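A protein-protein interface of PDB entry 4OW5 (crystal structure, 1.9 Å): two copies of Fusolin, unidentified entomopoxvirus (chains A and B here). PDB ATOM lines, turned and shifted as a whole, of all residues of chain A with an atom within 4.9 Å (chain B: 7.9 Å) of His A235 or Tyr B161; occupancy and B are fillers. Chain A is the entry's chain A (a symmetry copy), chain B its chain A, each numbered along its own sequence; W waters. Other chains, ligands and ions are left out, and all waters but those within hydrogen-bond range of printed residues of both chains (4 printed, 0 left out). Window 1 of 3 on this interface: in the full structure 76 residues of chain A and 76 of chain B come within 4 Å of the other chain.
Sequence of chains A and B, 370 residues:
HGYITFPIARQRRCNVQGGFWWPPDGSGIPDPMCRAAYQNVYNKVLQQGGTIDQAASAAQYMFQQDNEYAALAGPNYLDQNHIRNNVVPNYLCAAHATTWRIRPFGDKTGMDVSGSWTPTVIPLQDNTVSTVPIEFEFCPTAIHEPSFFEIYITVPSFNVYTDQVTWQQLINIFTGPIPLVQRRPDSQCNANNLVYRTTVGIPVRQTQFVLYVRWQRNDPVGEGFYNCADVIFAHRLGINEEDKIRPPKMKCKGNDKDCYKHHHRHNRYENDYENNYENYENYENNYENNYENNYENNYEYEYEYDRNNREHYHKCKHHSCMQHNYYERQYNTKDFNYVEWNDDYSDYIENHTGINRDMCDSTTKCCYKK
N of Ser B116 lies within hydrogen-bond range of SD of Met B33, at 3.6 Å. The backbone NH of Tyr B161 is in hydrogen-bond range of the side-chain amide oxygen of Asn B159 (3.0 Å). The backbone NH of Asn B159 lies within hydrogen-bond range of the side-chain carboxylate of Asp B163 (2.9 Å). OD1 of Asp B163 lies within hydrogen-bond range of OG1 of Thr B162, at 3.1 Å. The side-chain amide oxygen (OD1) of Asn A127 is in hydrogen-bond range of the backbone NH (N) of Arg A236. OE1 of Gln A206 lies within hydrogen-bond range of NE2 of His A235 (2.7 Å).
N of Asn A240 is in hydrogen-bond range of O of Ser B114 (2.9 Å). The side-chain amide nitrogen of Asn B159 is in hydrogen-bond range of the side-chain amide oxygen of Gln A206.
Of the 9 printed residues of chain A, 5 touch a printed residue of chain B. Hydrophobic or aromatic side chains of chain A that line the printed part of chain B: His A235 and Leu A237. Of the 17 printed residues of chain B, 6 touch a printed residue of chain A. Among the printed residues, no Asp or Glu carboxylate lies within 4 Å of a Lys or Arg side-chain nitrogen of the other chain.
Of the printed residues of chain B, Gln A206 touches Asn B159 and Thr B207. His A235 touches just one residue of chain B: Tyr B161. Printed residues of chain A within 4 Å of Ser B114: Asn A240 (2.9 Å). Gly B115 touches none of the printed residues of chain A. Trp B117 touches none of the printed residues of chain A. Printed residues of chain A within 4 Å of Tyr B161: Asn A127 (3.8 Å), His A235 (3.3 Å) and Asn A240 (3.6 Å). Of the printed residues of chain A, Thr B207 touches Gln A206. The nearest residue of chain B that does not touch His A235 is Asn B159 (4.8 Å). The nearest printed residue of chain A that does not touch Thr B207 is His A235 (7.1 Å).
Among the printed residues, pairs that only touch across the chains: His A235 with Tyr B161, Asn A240 with Thr B162, Asn A240 with Tyr B161, Leu A237 with Ser B116, Asn A127 with Thr B162, Gln A206 with Thr B207 and Asn A127 with Tyr B161.
Water W4 lies within hydrogen-bond range of O of Arg A236 (2.6 Å), ND2 of Asn A127 (3.3 Å) and N of Ser B116 (3.4 Å). Water W3 lies within hydrogen-bond range of O of Asn A127, ND2 of Asn B159, OE1 of Gln A206 and NE2 of His A235. Water W1 lies within hydrogen-bond range of the backbone carbonyl oxygen of Tyr B161 and the side-chain amide nitrogen of Asn A127. Water W2 bridges the side-chain amide nitrogen of Asn B159 and the side-chain amide nitrogen of Gln A206.
No position is printed for both chains. Of the 9 pairs that touch across the chains among the printed residues, none has its exchanged pair printed and touching as well.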
ATOM      1  N   LEU A 124      28.117  14.803 -27.766  1.00  0.00           N
ATOM      2  CA  LEU A 124      27.800  15.708 -28.861  1.00  0.00           C
ATOM      3  C   LEU A 124      29.106  16.302 -29.392  1.00  0.00           C
ATOM      4  O   LEU A 124      29.918  16.770 -28.600  1.00  0.00           O
ATOM      5  CB  LEU A 124      26.869  16.833 -28.388  1.00  0.00           C
ATOM      6  CG  LEU A 124      25.482  16.429 -27.924  1.00  0.00           C
ATOM      7  CD1 LEU A 124      24.749  17.599 -27.319  1.00  0.00           C
ATOM      8  CD2 LEU A 124      24.674  15.829 -29.041  1.00  0.00           C
ATOM      9  N   ASN A 127      27.223  21.291 -29.617  1.00  0.00           N
ATOM     10  CA  ASN A 127      26.042  21.447 -28.781  1.00  0.00           C
ATOM     11  C   ASN A 127      24.861  22.126 -29.475  1.00  0.00           C
ATOM     12  O   ASN A 127      23.758  22.014 -28.966  1.00  0.00           O
ATOM     13  CB  ASN A 127      26.395  22.207 -27.546  1.00  0.00           C
ATOM     14  CG  ASN A 127      27.384  21.468 -26.684  1.00  0.00           C
ATOM     15  OD1 ASN A 127      27.494  20.235 -26.728  1.00  0.00           O
ATOM     16  ND2 ASN A 127      28.165  22.194 -25.930  1.00  0.00           N
ATOM     17  N   GLN A 206      18.100  17.980 -23.706  1.00  0.00           N
ATOM     18  CA  GLN A 206      19.021  18.525 -22.717  1.00  0.00           C
ATOM     19  C   GLN A 206      18.959  17.730 -21.418  1.00  0.00           C
ATOM     20  O   GLN A 206      19.636  18.079 -20.485  1.00  0.00           O
ATOM     21  CB  GLN A 206      18.665  20.010 -22.471  1.00  0.00           C
ATOM     22  CG  GLN A 206      18.579  20.834 -23.771  1.00  0.00           C
ATOM     23  CD  GLN A 206      19.809  20.698 -24.651  1.00  0.00           C
ATOM     24  OE1 GLN A 206      20.944  20.741 -24.172  1.00  0.00           O
ATOM     25  NE2 GLN A 206      19.627  20.596 -25.965  1.00  0.00           N
ATOM     26  N   PHE A 233      22.513  12.754 -23.883  1.00  0.00           N
ATOM     27  CA  PHE A 233      23.529  13.391 -24.690  1.00  0.00           C
ATOM     28  C   PHE A 233      24.527  14.045 -23.726  1.00  0.00           C
ATOM     29  O   PHE A 233      24.105  14.619 -22.727  1.00  0.00           O
ATOM     30  CB  PHE A 233      22.892  14.415 -25.657  1.00  0.00           C
ATOM     31  CG  PHE A 233      22.182  13.717 -26.785  1.00  0.00           C
ATOM     32  CD1 PHE A 233      22.893  13.007 -27.732  1.00  0.00           C
ATOM     33  CD2 PHE A 233      20.800  13.772 -26.902  1.00  0.00           C
ATOM     34  CE1 PHE A 233      22.246  12.321 -28.743  1.00  0.00           C
ATOM     35  CE2 PHE A 233      20.154  13.122 -27.947  1.00  0.00           C
ATOM     36  CZ  PHE A 233      20.891  12.421 -28.882  1.00  0.00           C
ATOM     37  N   ALA A 234      25.821  13.919 -23.975  1.00  0.00           N
ATOM     38  CA  ALA A 234      26.845  14.573 -23.165  1.00  0.00           C
ATOM     39  C   ALA A 234      27.348  15.800 -23.937  1.00  0.00           C
ATOM     40  O   ALA A 234      27.756  15.686 -25.094  1.00  0.00           O
ATOM     41  CB  ALA A 234      27.973  13.627 -22.827  1.00  0.00           C
ATOM     42  N   HIS A 235      27.241  16.977 -23.338  1.00  0.00           N
ATOM     43  CA  HIS A 235      27.634  18.212 -24.031  1.00  0.00           C
ATOM     44  C   HIS A 235      29.112  18.392 -24.117  1.00  0.00           C
ATOM     45  O   HIS A 235      29.839  18.049 -23.192  1.00  0.00           O
ATOM     46  CB  HIS A 235      27.055  19.428 -23.328  1.00  0.00           C
ATOM     47  CG  HIS A 235      25.569  19.497 -23.373  1.00  0.00           C
ATOM     48  ND1 HIS A 235      24.801  19.199 -22.257  1.00  0.00           N
ATOM     49  CD2 HIS A 235      24.753  19.874 -24.383  1.00  0.00           C
ATOM     50  CE1 HIS A 235      23.541  19.354 -22.641  1.00  0.00           C
ATOM     51  NE2 HIS A 235      23.471  19.768 -23.914  1.00  0.00           N
ATOM     52  N   ARG A 236      29.565  19.002 -25.182  1.00  0.00           N
ATOM     53  CA  ARG A 236      30.961  19.368 -25.324  1.00  0.00           C
ATOM     54  C   ARG A 236      31.219  20.579 -24.384  1.00  0.00           C
ATOM     55  O   ARG A 236      30.373  21.478 -24.244  1.00  0.00           O
ATOM     56  CB  ARG A 236      31.313  19.698 -26.784  1.00  0.00           C
ATOM     57  CG  ARG A 236      32.815  19.826 -27.010  1.00  0.00           C
ATOM     58  CD  ARG A 236      33.197  19.848 -28.486  1.00  0.00           C
ATOM     59  NE  ARG A 236      33.709  21.142 -28.953  1.00  0.00           N
ATOM     60  CZ  ARG A 236      34.099  21.395 -30.200  1.00  0.00           C
ATOM     61  NH1 ARG A 236      34.040  20.445 -31.132  1.00  0.00           N
ATOM     62  NH2 ARG A 236      34.551  22.600 -30.529  1.00  0.00           N
ATOM     63  N   LEU A 237      32.366  20.592 -23.759  1.00  0.00           N
ATOM     64  CA  LEU A 237      32.756  21.655 -22.838  1.00  0.00           C
ATOM     65  C   LEU A 237      33.530  22.779 -23.555  1.00  0.00           C
ATOM     66  O   LEU A 237      34.190  22.563 -24.558  1.00  0.00           O
ATOM     67  CB  LEU A 237      33.615  21.071 -21.699  1.00  0.00           C
ATOM     68  CG  LEU A 237      32.965  19.965 -20.854  1.00  0.00           C
ATOM     69  CD1 LEU A 237      33.868  19.542 -19.719  1.00  0.00           C
ATOM     70  CD2 LEU A 237      31.638  20.410 -20.276  1.00  0.00           C
ATOM     71  N   ASN A 240      31.003  28.120 -26.796  1.00  0.00           N
ATOM     72  CA  ASN A 240      30.251  27.853 -28.010  1.00  0.00           C
ATOM     73  C   ASN A 240      31.034  28.505 -29.139  1.00  0.00           C
ATOM     74  O   ASN A 240      31.249  29.715 -29.112  1.00  0.00           O
ATOM     75  CB  ASN A 240      28.839  28.448 -27.874  1.00  0.00           C
ATOM     76  CG  ASN A 240      27.893  28.175 -29.017  1.00  0.00           C
ATOM     77  OD1 ASN A 240      28.222  27.480 -29.961  1.00  0.00           O
ATOM     78  ND2 ASN A 240      26.706  28.784 -29.010  1.00  0.00           N
ATOM     79  N   MET B  33      35.512  28.657 -19.227  1.00  0.00           N
ATOM     80  CA  MET B  33      34.577  29.711 -19.579  1.00  0.00           C
ATOM     81  C   MET B  33      35.061  31.047 -19.068  1.00  0.00           C
ATOM     82  O   MET B  33      34.968  31.995 -19.829  1.00  0.00           O
ATOM     83  CB  MET B  33      33.152  29.383 -19.132  1.00  0.00           C
ATOM     84  CG  MET B  33      32.535  28.235 -19.900  1.00  0.00           C
ATOM     85  SD  MET B  33      32.621  28.392 -21.707  1.00  0.00           S
ATOM     86  CE  MET B  33      31.706  29.854 -21.947  1.00  0.00           C
ATOM     87  N   VAL B 113      29.123  35.201 -23.355  1.00  0.00           N
ATOM     88  CA  VAL B 113      29.317  34.115 -24.284  1.00  0.00           C
ATOM     89  C   VAL B 113      28.579  32.881 -23.717  1.00  0.00           C
ATOM     90  O   VAL B 113      28.393  32.771 -22.519  1.00  0.00           O
ATOM     91  CB  VAL B 113      30.801  33.797 -24.595  1.00  0.00           C
ATOM     92  CG1 VAL B 113      31.539  35.001 -25.172  1.00  0.00           C
ATOM     93  CG2 VAL B 113      31.511  33.228 -23.394  1.00  0.00           C
ATOM     94  N   SER B 114      28.196  31.964 -24.579  1.00  0.00           N
ATOM     95  CA  SER B 114      27.525  30.744 -24.185  1.00  0.00           C
ATOM     96  C   SER B 114      28.550  29.607 -24.116  1.00  0.00           C
ATOM     97  O   SER B 114      29.619  29.683 -24.717  1.00  0.00           O
ATOM     98  CB  SER B 114      26.376  30.427 -25.143  1.00  0.00           C
ATOM     99  OG  SER B 114      26.798  30.347 -26.485  1.00  0.00           O
ATOM    100  N   GLY B 115      28.241  28.626 -23.306  1.00  0.00           N
ATOM    101  CA  GLY B 115      29.097  27.487 -23.052  1.00  0.00           C
ATOM    102  C   GLY B 115      28.899  26.865 -21.692  1.00  0.00           C
ATOM    103  O   GLY B 115      27.901  27.146 -21.007  1.00  0.00           O
ATOM    104  N   SER B 116      29.900  26.056 -21.277  1.00  0.00           N
ATOM    105  CA  SER B 116      29.853  25.225 -20.073  1.00  0.00           C
ATOM    106  C   SER B 116      30.204  26.001 -18.798  1.00  0.00           C
ATOM    107  O   SER B 116      31.121  25.608 -18.068  1.00  0.00           O
ATOM    108  CB  SER B 116      30.791  24.030 -20.240  1.00  0.00           C
ATOM    109  OG  SER B 116      32.105  24.427 -20.602  1.00  0.00           O
ATOM    110  N   TRP B 117      29.450  27.080 -18.500  1.00  0.00           N
ATOM    111  CA  TRP B 117      29.700  27.900 -17.312  1.00  0.00           C
ATOM    112  C   TRP B 117      29.613  27.034 -16.069  1.00  0.00           C
ATOM    113  O   TRP B 117      28.732  26.191 -16.014  1.00  0.00           O
ATOM    114  CB  TRP B 117      28.718  29.068 -17.215  1.00  0.00           C
ATOM    115  CG  TRP B 117      28.985  30.135 -18.233  1.00  0.00           C
ATOM    116  CD1 TRP B 117      28.366  30.310 -19.438  1.00  0.00           C
ATOM    117  CD2 TRP B 117      30.007  31.124 -18.161  1.00  0.00           C
ATOM    118  NE1 TRP B 117      28.860  31.437 -20.055  1.00  0.00           N
ATOM    119  CE2 TRP B 117      29.932  31.892 -19.343  1.00  0.00           C
ATOM    120  CE3 TRP B 117      30.971  31.457 -17.194  1.00  0.00           C
ATOM    121  CZ2 TRP B 117      30.779  32.961 -19.581  1.00  0.00           C
ATOM    122  CZ3 TRP B 117      31.815  32.523 -17.438  1.00  0.00           C
ATOM    123  CH2 TRP B 117      31.705  33.266 -18.606  1.00  0.00           C
ATOM    124  N   PRO B 119      28.527  25.860 -12.640  1.00  0.00           N
ATOM    125  CA  PRO B 119      27.443  26.245 -11.747  1.00  0.00           C
ATOM    126  C   PRO B 119      27.684  25.919 -10.309  1.00  0.00           C
ATOM    127  O   PRO B 119      28.483  25.064  -9.976  1.00  0.00           O
ATOM    128  CB  PRO B 119      26.296  25.385 -12.264  1.00  0.00           C
ATOM    129  CG  PRO B 119      27.005  24.052 -12.587  1.00  0.00           C
ATOM    130  CD  PRO B 119      28.361  24.469 -13.120  1.00  0.00           C
ATOM    131  N   PHE B 158      15.715  27.259 -21.594  1.00  0.00           N
ATOM    132  CA  PHE B 158      17.021  27.903 -21.668  1.00  0.00           C
ATOM    133  C   PHE B 158      18.131  26.856 -21.681  1.00  0.00           C
ATOM    134  O   PHE B 158      18.162  25.939 -20.857  1.00  0.00           O
ATOM    135  CB  PHE B 158      17.211  28.871 -20.481  1.00  0.00           C
ATOM    136  CG  PHE B 158      18.589  29.475 -20.347  1.00  0.00           C
ATOM    137  CD1 PHE B 158      18.987  30.521 -21.166  1.00  0.00           C
ATOM    138  CD2 PHE B 158      19.515  28.943 -19.460  1.00  0.00           C
ATOM    139  CE1 PHE B 158      20.288  31.026 -21.101  1.00  0.00           C
ATOM    140  CE2 PHE B 158      20.798  29.475 -19.366  1.00  0.00           C
ATOM    141  CZ  PHE B 158      21.178  30.505 -20.198  1.00  0.00           C
ATOM    142  N   ASN B 159      19.085  27.051 -22.572  1.00  0.00           N
ATOM    143  CA  ASN B 159      20.219  26.144 -22.729  1.00  0.00           C
ATOM    144  C   ASN B 159      21.496  26.982 -22.590  1.00  0.00           C
ATOM    145  O   ASN B 159      21.837  27.730 -23.501  1.00  0.00           O
ATOM    146  CB  ASN B 159      20.106  25.441 -24.083  1.00  0.00           C
ATOM    147  CG  ASN B 159      21.193  24.461 -24.383  1.00  0.00           C
ATOM    148  OD1 ASN B 159      22.295  24.540 -23.846  1.00  0.00           O
ATOM    149  ND2 ASN B 159      20.968  23.616 -25.356  1.00  0.00           N
ATOM    150  N   VAL B 160      22.185  26.863 -21.447  1.00  0.00           N
ATOM    151  CA  VAL B 160      23.380  27.657 -21.147  1.00  0.00           C
ATOM    152  C   VAL B 160      24.484  27.422 -22.186  1.00  0.00           C
ATOM    153  O   VAL B 160      25.250  28.347 -22.484  1.00  0.00           O
ATOM    154  CB  VAL B 160      23.902  27.390 -19.709  1.00  0.00           C
ATOM    155  CG1 VAL B 160      24.571  26.025 -19.592  1.00  0.00           C
ATOM    156  CG2 VAL B 160      24.837  28.503 -19.252  1.00  0.00           C
ATOM    157  N   TYR B 161      24.549  26.209 -22.754  1.00  0.00           N
ATOM    158  CA  TYR B 161      25.597  25.853 -23.712  1.00  0.00           C
ATOM    159  C   TYR B 161      25.506  26.632 -25.013  1.00  0.00           C
ATOM    160  O   TYR B 161      26.512  26.734 -25.705  1.00  0.00           O
ATOM    161  CB  TYR B 161      25.555  24.345 -24.029  1.00  0.00           C
ATOM    162  CG  TYR B 161      25.814  23.472 -22.831  1.00  0.00           C
ATOM    163  CD1 TYR B 161      27.109  23.222 -22.394  1.00  0.00           C
ATOM    164  CD2 TYR B 161      24.763  22.902 -22.121  1.00  0.00           C
ATOM    165  CE1 TYR B 161      27.353  22.463 -21.251  1.00  0.00           C
ATOM    166  CE2 TYR B 161      24.988  22.184 -20.955  1.00  0.00           C
ATOM    167  CZ  TYR B 161      26.288  21.984 -20.508  1.00  0.00           C
ATOM    168  OH  TYR B 161      26.547  21.179 -19.429  1.00  0.00           O
ATOM    169  N   THR B 162      24.310  27.086 -25.395  1.00  0.00           N
ATOM    170  CA  THR B 162      24.129  27.734 -26.699  1.00  0.00           C
ATOM    171  C   THR B 162      23.455  29.101 -26.690  1.00  0.00           C
ATOM    172  O   THR B 162      23.509  29.783 -27.717  1.00  0.00           O
ATOM    173  CB  THR B 162      23.294  26.798 -27.595  1.00  0.00           C
ATOM    174  OG1 THR B 162      21.964  26.701 -27.064  1.00  0.00           O
ATOM    175  CG2 THR B 162      23.890  25.412 -27.704  1.00  0.00           C
ATOM    176  N   ASP B 163      22.812  29.512 -25.597  1.00  0.00           N
ATOM    177  CA  ASP B 163      22.018  30.730 -25.608  1.00  0.00           C
ATOM    178  C   ASP B 163      22.600  31.877 -24.836  1.00  0.00           C
ATOM    179  O   ASP B 163      23.123  31.671 -23.742  1.00  0.00           O
ATOM    180  CB  ASP B 163      20.670  30.477 -24.938  1.00  0.00           C
ATOM    181  CG  ASP B 163      19.832  29.360 -25.490  1.00  0.00           C
ATOM    182  OD1 ASP B 163      19.952  29.073 -26.718  1.00  0.00           O
ATOM    183  OD2 ASP B 163      18.905  28.922 -24.777  1.00  0.00           O
ATOM    184  N   GLN B 164      22.300  33.090 -25.299  1.00  0.00           N
ATOM    185  CA  GLN B 164      22.527  34.302 -24.530  1.00  0.00           C
ATOM    186  C   GLN B 164      21.309  34.410 -23.655  1.00  0.00           C
ATOM    187  O   GLN B 164      20.243  33.988 -24.083  1.00  0.00           O
ATOM    188  CB  GLN B 164      22.680  35.565 -25.386  1.00  0.00           C
ATOM    189  CG  GLN B 164      24.098  35.958 -25.733  1.00  0.00           C
ATOM    190  CD  GLN B 164      24.673  35.018 -26.724  1.00  0.00           C
ATOM    191  OE1 GLN B 164      24.156  34.890 -27.854  1.00  0.00           O
ATOM    192  NE2 GLN B 164      25.733  34.324 -26.344  1.00  0.00           N
ATOM    193  N   THR B 207      17.668  20.963 -15.710  1.00  0.00           N
ATOM    194  CA  THR B 207      18.843  21.373 -16.474  1.00  0.00           C
ATOM    195  C   THR B 207      19.556  22.514 -15.765  1.00  0.00           C
ATOM    196  O   THR B 207      18.974  23.185 -14.902  1.00  0.00           O
ATOM    197  CB  THR B 207      18.383  21.847 -17.859  1.00  0.00           C
ATOM    198  OG1 THR B 207      17.407  22.869 -17.660  1.00  0.00           O
ATOM    199  CG2 THR B 207      17.792  20.737 -18.699  1.00  0.00           C
ATOM    200  N   GLN B 208      20.771  22.788 -16.202  1.00  0.00           N
ATOM    201  CA  GLN B 208      21.532  23.902 -15.681  1.00  0.00           C
ATOM    202  C   GLN B 208      20.804  25.193 -16.069  1.00  0.00           C
ATOM    203  O   GLN B 208      20.294  25.304 -17.180  1.00  0.00           O
ATOM    204  CB  GLN B 208      22.962  23.867 -16.200  1.00  0.00           C
ATOM    205  CG  GLN B 208      23.760  25.017 -15.698  1.00  0.00           C
ATOM    206  CD  GLN B 208      25.230  24.890 -15.908  1.00  0.00           C
ATOM    207  OE1 GLN B 208      25.787  23.796 -16.065  1.00  0.00           O
ATOM    208  NE2 GLN B 208      25.886  26.013 -15.958  1.00  0.00           N
ATOM    209  N   ILE B 232      22.711  24.484 -10.851  1.00  0.00           N
ATOM    210  CA  ILE B 232      22.189  23.195 -11.249  1.00  0.00           C
ATOM    211  C   ILE B 232      21.765  22.418 -10.015  1.00  0.00           C
ATOM    212  O   ILE B 232      22.429  22.461  -8.986  1.00  0.00           O
ATOM    213  CB  ILE B 232      23.185  22.372 -12.116  1.00  0.00           C
ATOM    214  CG1 ILE B 232      22.422  21.305 -12.915  1.00  0.00           C
ATOM    215  CG2 ILE B 232      24.340  21.766 -11.305  1.00  0.00           C
ATOM    216  CD1 ILE B 232      23.316  20.490 -13.905  1.00  0.00           C
HETATM  217  O   HOH W   1      28.548  25.052 -26.385  1.00  0.00           O
HETATM  218  O   HOH W   2      18.509  23.838 -26.624  1.00  0.00           O
HETATM  219  O   HOH W   3      22.805  21.557 -26.453  1.00  0.00           O
HETATM  220  O   HOH W   4      30.112  24.099 -24.060  1.00  0.00           O
